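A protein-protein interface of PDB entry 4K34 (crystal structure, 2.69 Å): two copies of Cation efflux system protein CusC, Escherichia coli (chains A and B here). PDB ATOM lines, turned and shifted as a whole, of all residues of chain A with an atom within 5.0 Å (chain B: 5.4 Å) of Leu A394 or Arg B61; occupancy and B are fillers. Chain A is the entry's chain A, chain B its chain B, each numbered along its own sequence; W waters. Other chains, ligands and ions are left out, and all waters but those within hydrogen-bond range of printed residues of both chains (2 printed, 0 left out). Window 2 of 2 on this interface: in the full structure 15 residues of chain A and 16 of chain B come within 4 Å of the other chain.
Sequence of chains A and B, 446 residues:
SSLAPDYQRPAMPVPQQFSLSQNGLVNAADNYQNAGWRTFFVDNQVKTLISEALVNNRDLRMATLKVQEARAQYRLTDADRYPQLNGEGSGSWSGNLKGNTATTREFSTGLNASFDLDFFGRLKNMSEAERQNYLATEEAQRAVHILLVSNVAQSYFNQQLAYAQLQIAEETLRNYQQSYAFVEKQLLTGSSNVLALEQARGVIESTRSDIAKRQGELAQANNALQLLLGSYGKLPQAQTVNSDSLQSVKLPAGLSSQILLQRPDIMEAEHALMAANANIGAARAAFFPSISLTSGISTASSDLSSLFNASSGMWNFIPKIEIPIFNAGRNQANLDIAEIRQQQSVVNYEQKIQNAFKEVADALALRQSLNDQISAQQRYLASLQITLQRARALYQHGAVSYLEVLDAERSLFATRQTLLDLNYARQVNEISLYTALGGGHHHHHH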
ATOM      1  N   ARG A 390       6.719 -11.418 -22.277  1.00  0.00           N
ATOM      2  CA  ARG A 390       8.075 -11.775 -22.635  1.00  0.00           C
ATOM      3  C   ARG A 390       8.397 -13.205 -22.216  1.00  0.00           C
ATOM      4  O   ARG A 390       8.993 -13.976 -22.988  1.00  0.00           O
ATOM      5  CB  ARG A 390       9.051 -10.754 -22.067  1.00  0.00           C
ATOM      6  CG  ARG A 390       8.781  -9.357 -22.625  1.00  0.00           C
ATOM      7  CD  ARG A 390      10.021  -8.514 -22.768  1.00  0.00           C
ATOM      8  NE  ARG A 390      10.423  -7.904 -21.509  1.00  0.00           N
ATOM      9  CZ  ARG A 390      10.561  -6.593 -21.311  1.00  0.00           C
ATOM     10  NH1 ARG A 390      10.335  -5.734 -22.304  1.00  0.00           N
ATOM     11  NH2 ARG A 390      10.941  -6.143 -20.114  1.00  0.00           N
ATOM     12  N   ALA A 391       7.956 -13.570 -21.016  1.00  0.00           N
ATOM     13  CA  ALA A 391       8.124 -14.934 -20.528  1.00  0.00           C
ATOM     14  C   ALA A 391       7.406 -15.958 -21.424  1.00  0.00           C
ATOM     15  O   ALA A 391       7.925 -17.041 -21.661  1.00  0.00           O
ATOM     16  CB  ALA A 391       7.653 -15.046 -19.094  1.00  0.00           C
ATOM     17  N   ARG A 392       6.221 -15.613 -21.923  1.00  0.00           N
ATOM     18  CA  ARG A 392       5.480 -16.506 -22.814  1.00  0.00           C
ATOM     19  C   ARG A 392       6.184 -16.735 -24.149  1.00  0.00           C
ATOM     20  O   ARG A 392       6.275 -17.870 -24.634  1.00  0.00           O
ATOM     21  CB  ARG A 392       4.081 -15.974 -23.067  1.00  0.00           C
ATOM     22  CG  ARG A 392       3.169 -16.192 -21.917  1.00  0.00           C
ATOM     23  CD  ARG A 392       1.817 -15.566 -22.134  1.00  0.00           C
ATOM     24  NE  ARG A 392       0.893 -16.167 -21.183  1.00  0.00           N
ATOM     25  CZ  ARG A 392      -0.160 -15.556 -20.653  1.00  0.00           C
ATOM     26  NH1 ARG A 392      -0.444 -14.299 -20.983  1.00  0.00           N
ATOM     27  NH2 ARG A 392      -0.927 -16.209 -19.787  1.00  0.00           N
ATOM     28  N   ALA A 393       6.664 -15.652 -24.742  1.00  0.00           N
ATOM     29  CA  ALA A 393       7.468 -15.753 -25.946  1.00  0.00           C
ATOM     30  C   ALA A 393       8.737 -16.596 -25.700  1.00  0.00           C
ATOM     31  O   ALA A 393       9.079 -17.477 -26.498  1.00  0.00           O
ATOM     32  CB  ALA A 393       7.807 -14.362 -26.469  1.00  0.00           C
ATOM     33  N   LEU A 394       9.426 -16.347 -24.588  1.00  0.00           N
ATOM     34  CA  LEU A 394      10.612 -17.127 -24.274  1.00  0.00           C
ATOM     35  C   LEU A 394      10.292 -18.604 -24.089  1.00  0.00           C
ATOM     36  O   LEU A 394      11.114 -19.470 -24.374  1.00  0.00           O
ATOM     37  CB  LEU A 394      11.323 -16.569 -23.047  1.00  0.00           C
ATOM     38  CG  LEU A 394      12.158 -15.342 -23.410  1.00  0.00           C
ATOM     39  CD1 LEU A 394      12.786 -14.729 -22.182  1.00  0.00           C
ATOM     40  CD2 LEU A 394      13.218 -15.709 -24.436  1.00  0.00           C
ATOM     41  N   TYR A 395       9.091 -18.890 -23.615  1.00  0.00           N
ATOM     42  CA  TYR A 395       8.693 -20.263 -23.360  1.00  0.00           C
ATOM     43  C   TYR A 395       8.545 -20.978 -24.694  1.00  0.00           C
ATOM     44  O   TYR A 395       8.967 -22.121 -24.865  1.00  0.00           O
ATOM     45  CB  TYR A 395       7.383 -20.300 -22.581  1.00  0.00           C
ATOM     46  CG  TYR A 395       6.774 -21.668 -22.568  1.00  0.00           C
ATOM     47  CD1 TYR A 395       7.332 -22.688 -21.812  1.00  0.00           C
ATOM     48  CD2 TYR A 395       5.650 -21.952 -23.332  1.00  0.00           C
ATOM     49  CE1 TYR A 395       6.783 -23.951 -21.809  1.00  0.00           C
ATOM     50  CE2 TYR A 395       5.091 -23.213 -23.341  1.00  0.00           C
ATOM     51  CZ  TYR A 395       5.660 -24.213 -22.578  1.00  0.00           C
ATOM     52  OH  TYR A 395       5.099 -25.476 -22.582  1.00  0.00           O
ATOM     53  N   GLN A 396       7.961 -20.265 -25.643  1.00  0.00           N
ATOM     54  CA  GLN A 396       7.783 -20.754 -26.999  1.00  0.00           C
ATOM     55  C   GLN A 396       9.103 -21.086 -27.705  1.00  0.00           C
ATOM     56  O   GLN A 396       9.106 -21.785 -28.715  1.00  0.00           O
ATOM     57  CB  GLN A 396       7.026 -19.716 -27.822  1.00  0.00           C
ATOM     58  CG  GLN A 396       5.821 -20.275 -28.502  1.00  0.00           C
ATOM     59  CD  GLN A 396       4.716 -20.602 -27.530  1.00  0.00           C
ATOM     60  OE1 GLN A 396       4.320 -21.765 -27.383  1.00  0.00           O
ATOM     61  NE2 GLN A 396       4.197 -19.573 -26.859  1.00  0.00           N
ATOM     62  N   HIS A 397      10.214 -20.570 -27.186  1.00  0.00           N
ATOM     63  CA  HIS A 397      11.528 -20.856 -27.744  1.00  0.00           C
ATOM     64  C   HIS A 397      12.323 -21.853 -26.897  1.00  0.00           C
ATOM     65  O   HIS A 397      13.517 -22.052 -27.138  1.00  0.00           O
ATOM     66  CB  HIS A 397      12.342 -19.571 -27.895  1.00  0.00           C
ATOM     67  CG  HIS A 397      11.854 -18.669 -28.984  1.00  0.00           C
ATOM     68  ND1 HIS A 397      10.574 -18.163 -29.013  1.00  0.00           N
ATOM     69  CD2 HIS A 397      12.481 -18.176 -30.079  1.00  0.00           C
ATOM     70  CE1 HIS A 397      10.430 -17.396 -30.083  1.00  0.00           C
ATOM     71  NE2 HIS A 397      11.571 -17.389 -30.746  1.00  0.00           N
ATOM     72  N   GLY A 398      11.676 -22.465 -25.905  1.00  0.00           N
ATOM     73  CA  GLY A 398      12.359 -23.385 -25.008  1.00  0.00           C
ATOM     74  C   GLY A 398      13.295 -22.686 -24.027  1.00  0.00           C
ATOM     75  O   GLY A 398      14.007 -23.330 -23.254  1.00  0.00           O
ATOM     76  N   ALA A 399      13.278 -21.355 -24.037  1.00  0.00           N
ATOM     77  CA  ALA A 399      14.177 -20.569 -23.196  1.00  0.00           C
ATOM     78  C   ALA A 399      13.823 -20.564 -21.699  1.00  0.00           C
ATOM     79  O   ALA A 399      14.695 -20.313 -20.877  1.00  0.00           O
ATOM     80  CB  ALA A 399      14.296 -19.148 -23.730  1.00  0.00           C
ATOM     81  N   VAL A 400      12.560 -20.823 -21.347  1.00  0.00           N
ATOM     82  CA  VAL A 400      12.153 -20.943 -19.932  1.00  0.00           C
ATOM     83  C   VAL A 400      11.119 -22.044 -19.669  1.00  0.00           C
ATOM     84  O   VAL A 400      10.329 -22.406 -20.536  1.00  0.00           O
ATOM     85  CB  VAL A 400      11.571 -19.629 -19.334  1.00  0.00           C
ATOM     86  CG1 VAL A 400      12.634 -18.570 -19.195  1.00  0.00           C
ATOM     87  CG2 VAL A 400      10.418 -19.117 -20.163  1.00  0.00           C
ATOM     88  N   ASP B  59      15.680 -19.613 -11.875  1.00  0.00           N
ATOM     89  CA  ASP B  59      15.824 -19.624 -13.324  1.00  0.00           C
ATOM     90  C   ASP B  59      16.604 -18.398 -13.811  1.00  0.00           C
ATOM     91  O   ASP B  59      16.170 -17.256 -13.641  1.00  0.00           O
ATOM     92  CB  ASP B  59      14.455 -19.697 -13.997  1.00  0.00           C
ATOM     93  CG  ASP B  59      14.542 -20.049 -15.471  1.00  0.00           C
ATOM     94  OD1 ASP B  59      15.015 -19.194 -16.245  1.00  0.00           O
ATOM     95  OD2 ASP B  59      14.115 -21.167 -15.869  1.00  0.00           O
ATOM     96  N   LEU B  60      17.750 -18.669 -14.433  1.00  0.00           N
ATOM     97  CA  LEU B  60      18.675 -17.655 -14.902  1.00  0.00           C
ATOM     98  C   LEU B  60      18.106 -16.716 -15.972  1.00  0.00           C
ATOM     99  O   LEU B  60      18.353 -15.496 -15.933  1.00  0.00           O
ATOM    100  CB  LEU B  60      19.925 -18.333 -15.449  1.00  0.00           C
ATOM    101  CG  LEU B  60      21.189 -18.100 -14.645  1.00  0.00           C
ATOM    102  CD1 LEU B  60      20.867 -18.196 -13.171  1.00  0.00           C
ATOM    103  CD2 LEU B  60      22.235 -19.113 -15.041  1.00  0.00           C
ATOM    104  N   ARG B  61      17.380 -17.278 -16.941  1.00  0.00           N
ATOM    105  CA  ARG B  61      16.833 -16.475 -18.036  1.00  0.00           C
ATOM    106  C   ARG B  61      15.758 -15.513 -17.510  1.00  0.00           C
ATOM    107  O   ARG B  61      15.777 -14.316 -17.828  1.00  0.00           O
ATOM    108  CB  ARG B  61      16.292 -17.366 -19.158  1.00  0.00           C
ATOM    109  CG  ARG B  61      15.920 -16.616 -20.416  1.00  0.00           C
ATOM    110  CD  ARG B  61      17.131 -15.893 -20.993  1.00  0.00           C
ATOM    111  NE  ARG B  61      16.852 -15.226 -22.270  1.00  0.00           N
ATOM    112  CZ  ARG B  61      16.832 -15.832 -23.463  1.00  0.00           C
ATOM    113  NH1 ARG B  61      17.066 -17.136 -23.560  1.00  0.00           N
ATOM    114  NH2 ARG B  61      16.582 -15.131 -24.562  1.00  0.00           N
ATOM    115  N   MET B  62      14.839 -16.034 -16.695  1.00  0.00           N
ATOM    116  CA  MET B  62      13.896 -15.204 -15.948  1.00  0.00           C
ATOM    117  C   MET B  62      14.545 -14.038 -15.160  1.00  0.00           C
ATOM    118  O   MET B  62      14.024 -12.913 -15.169  1.00  0.00           O
ATOM    119  CB  MET B  62      13.051 -16.063 -15.002  1.00  0.00           C
ATOM    120  CG  MET B  62      12.025 -16.944 -15.702  1.00  0.00           C
ATOM    121  SD  MET B  62      10.952 -16.024 -16.837  1.00  0.00           S
ATOM    122  CE  MET B  62      10.089 -14.929 -15.690  1.00  0.00           C
ATOM    123  N   ALA B  63      15.665 -14.309 -14.487  1.00  0.00           N
ATOM    124  CA  ALA B  63      16.382 -13.279 -13.741  1.00  0.00           C
ATOM    125  C   ALA B  63      16.810 -12.140 -14.666  1.00  0.00           C
ATOM    126  O   ALA B  63      16.689 -10.956 -14.340  1.00  0.00           O
ATOM    127  CB  ALA B  63      17.581 -13.874 -13.035  1.00  0.00           C
ATOM    128  N   THR B  64      17.295 -12.527 -15.829  1.00  0.00           N
ATOM    129  CA  THR B  64      17.593 -11.615 -16.925  1.00  0.00           C
ATOM    130  C   THR B  64      16.392 -10.742 -17.338  1.00  0.00           C
ATOM    131  O   THR B  64      16.549  -9.552 -17.660  1.00  0.00           O
ATOM    132  CB  THR B  64      18.152 -12.437 -18.099  1.00  0.00           C
ATOM    133  OG1 THR B  64      19.579 -12.455 -18.005  1.00  0.00           O
ATOM    134  CG2 THR B  64      17.710 -11.910 -19.439  1.00  0.00           C
ATOM    135  N   LEU B  65      15.196 -11.315 -17.295  1.00  0.00           N
ATOM    136  CA  LEU B  65      13.977 -10.562 -17.608  1.00  0.00           C
ATOM    137  C   LEU B  65      13.661  -9.520 -16.553  1.00  0.00           C
ATOM    138  O   LEU B  65      13.302  -8.374 -16.856  1.00  0.00           O
ATOM    139  CB  LEU B  65      12.770 -11.501 -17.691  1.00  0.00           C
ATOM    140  CG  LEU B  65      12.492 -12.138 -19.034  1.00  0.00           C
ATOM    141  CD1 LEU B  65      10.997 -12.292 -19.188  1.00  0.00           C
ATOM    142  CD2 LEU B  65      13.091 -11.272 -20.131  1.00  0.00           C
ATOM    143  N   GLU B 128      19.204 -16.827 -30.474  1.00  0.00           N
ATOM    144  CA  GLU B 128      18.541 -17.498 -29.377  1.00  0.00           C
ATOM    145  C   GLU B 128      19.240 -18.799 -28.992  1.00  0.00           C
ATOM    146  O   GLU B 128      19.433 -19.081 -27.805  1.00  0.00           O
ATOM    147  CB  GLU B 128      17.073 -17.750 -29.732  1.00  0.00           C
ATOM    148  CG  GLU B 128      16.248 -18.317 -28.601  1.00  0.00           C
ATOM    149  CD  GLU B 128      16.450 -17.573 -27.286  1.00  0.00           C
ATOM    150  OE1 GLU B 128      16.677 -16.344 -27.311  1.00  0.00           O
ATOM    151  OE2 GLU B 128      16.380 -18.234 -26.228  1.00  0.00           O
ATOM    152  N   ARG B 131      22.395 -17.848 -27.080  1.00  0.00           N
ATOM    153  CA  ARG B 131      22.013 -17.455 -25.729  1.00  0.00           C
ATOM    154  C   ARG B 131      21.766 -18.622 -24.781  1.00  0.00           C
ATOM    155  O   ARG B 131      22.249 -18.612 -23.653  1.00  0.00           O
ATOM    156  CB  ARG B 131      20.804 -16.524 -25.763  1.00  0.00           C
ATOM    157  CG  ARG B 131      21.135 -15.187 -26.350  1.00  0.00           C
ATOM    158  CD  ARG B 131      20.013 -14.227 -26.149  1.00  0.00           C
ATOM    159  NE  ARG B 131      18.915 -14.529 -27.044  1.00  0.00           N
ATOM    160  CZ  ARG B 131      18.554 -13.763 -28.063  1.00  0.00           C
ATOM    161  NH1 ARG B 131      19.197 -12.633 -28.305  1.00  0.00           N
ATOM    162  NH2 ARG B 131      17.535 -14.125 -28.827  1.00  0.00           N
ATOM    163  N   GLN B 132      21.020 -19.624 -25.219  1.00  0.00           N
ATOM    164  CA  GLN B 132      20.717 -20.735 -24.318  1.00  0.00           C
ATOM    165  C   GLN B 132      21.967 -21.550 -23.994  1.00  0.00           C
ATOM    166  O   GLN B 132      22.112 -22.059 -22.881  1.00  0.00           O
ATOM    167  CB  GLN B 132      19.581 -21.601 -24.872  1.00  0.00           C
ATOM    168  CG  GLN B 132      18.392 -20.744 -25.258  1.00  0.00           C
ATOM    169  CD  GLN B 132      17.189 -21.535 -25.694  1.00  0.00           C
ATOM    170  OE1 GLN B 132      17.000 -22.687 -25.290  1.00  0.00           O
ATOM    171  NE2 GLN B 132      16.357 -20.917 -26.531  1.00  0.00           N
ATOM    172  N   LEU B 135      24.254 -19.399 -21.457  1.00  0.00           N
ATOM    173  CA  LEU B 135      23.748 -19.326 -20.094  1.00  0.00           C
ATOM    174  C   LEU B 135      23.962 -20.637 -19.350  1.00  0.00           C
ATOM    175  O   LEU B 135      23.575 -20.780 -18.185  1.00  0.00           O
ATOM    176  CB  LEU B 135      22.276 -18.890 -20.067  1.00  0.00           C
ATOM    177  CG  LEU B 135      22.010 -17.461 -20.566  1.00  0.00           C
ATOM    178  CD1 LEU B 135      20.541 -17.151 -20.531  1.00  0.00           C
ATOM    179  CD2 LEU B 135      22.787 -16.414 -19.795  1.00  0.00           C
HETATM  180  O   HOH W   1      10.306  -7.719 -18.302  1.00  0.00           O
HETATM  181  O   HOH W   2      17.635 -19.489 -21.951  1.00  0.00           O
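Water W1 lies within hydrogen-bond range of NH2 of Arg A390 and O of Leu B65.
Water W2 lies within hydrogen-bond range of NH1 of Arg B61 (2.9 Å) and O of Ala A399 (3.2 Å).
The side-chain amide nitrogen (NE2) of Gln B132 is in hydrogen-bond range of the backbone carbonyl oxygen (O) of His A397.
Among the printed residues, pairs that only touch across the chains: Arg A390 with Leu B65 (3.8 Å), Ala A391 with Leu B65 (3.8 Å), Leu A394 with Arg B61 (3.4 Å), Gly A398 with Gln B132 (3.7 Å), Ala A399 with Arg B61 (3.4 Å), Ala A399 with Glu B128 (3.4 Å), Ala A399 with Gln B132 (3.9 Å), Val A400 with Asp B59 (3.8 Å), Val A400 with Arg B61 (3.9 Å) and Val A400 with Met B62 (3.9 Å).
O of Ala A393 sits at hydrogen-bond distance from ND1 of His A397.
O of Leu A394 is in hydrogen-bond range of N of Ala A399.
The side-chain carboxylate of Asp B59 is in hydrogen-bond range of the backbone NH of Arg B61 (3.1 Å).
N of Met B62 is in hydrogen-bond range of OD1 of Asp B59 (3.2 Å).
The guanidinium group (NH1) of Arg B61 lies within salt-bridge range of the side-chain carboxylate (OE2) of Glu B128 (3.0 Å).
The guanidinium group (NH2) of Arg B131 is in salt-bridge range of the side-chain carboxylate (OE1) of Glu B128 (2.8 Å).
No position is printed for both chains.
Of the 11 pairs that touch across the chains among the printed residues, none has its exchanged pair printed and touching as well.
Leu A394 touches one residue of chain B.
Gln A396 touches none of the printed residues of chain B.
Of the printed residues of chain B, Gly A398 touches Gln B132 (3.7 Å).
Arg B61 touches three residues of chain A.
Printed residues of chain A within 4 Å of Met B62: Val A400 (3.9 Å).
Of the printed residues of chain A, Gln B132 touches His A397, Gly A398 and Ala A399.
The nearest printed residue of chain A that does not touch Arg B61 is Gly A398 (6.7 Å).
Of the 11 printed residues of chain B, 6 touch a printed residue of chain A.
Hydrophobic or aromatic side chains of chain B within 4 Å of the printed part of chain A: Met B62 and Leu B65.
Of the 11 printed residues of chain A, 7 touch a printed residue of chain B.
Printed residues of chain A that touch a printed residue of chain B: Arg A390, Ala A391, Leu A394, His A397, Gly A398, Ala A399 and Val A400.
Among the printed residues, 11 pairs touch across the chains.
Among the printed residues, no Asp or Glu carboxylate lies within 4 Å of a Lys or Arg side-chain nitrogen of the other chain.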
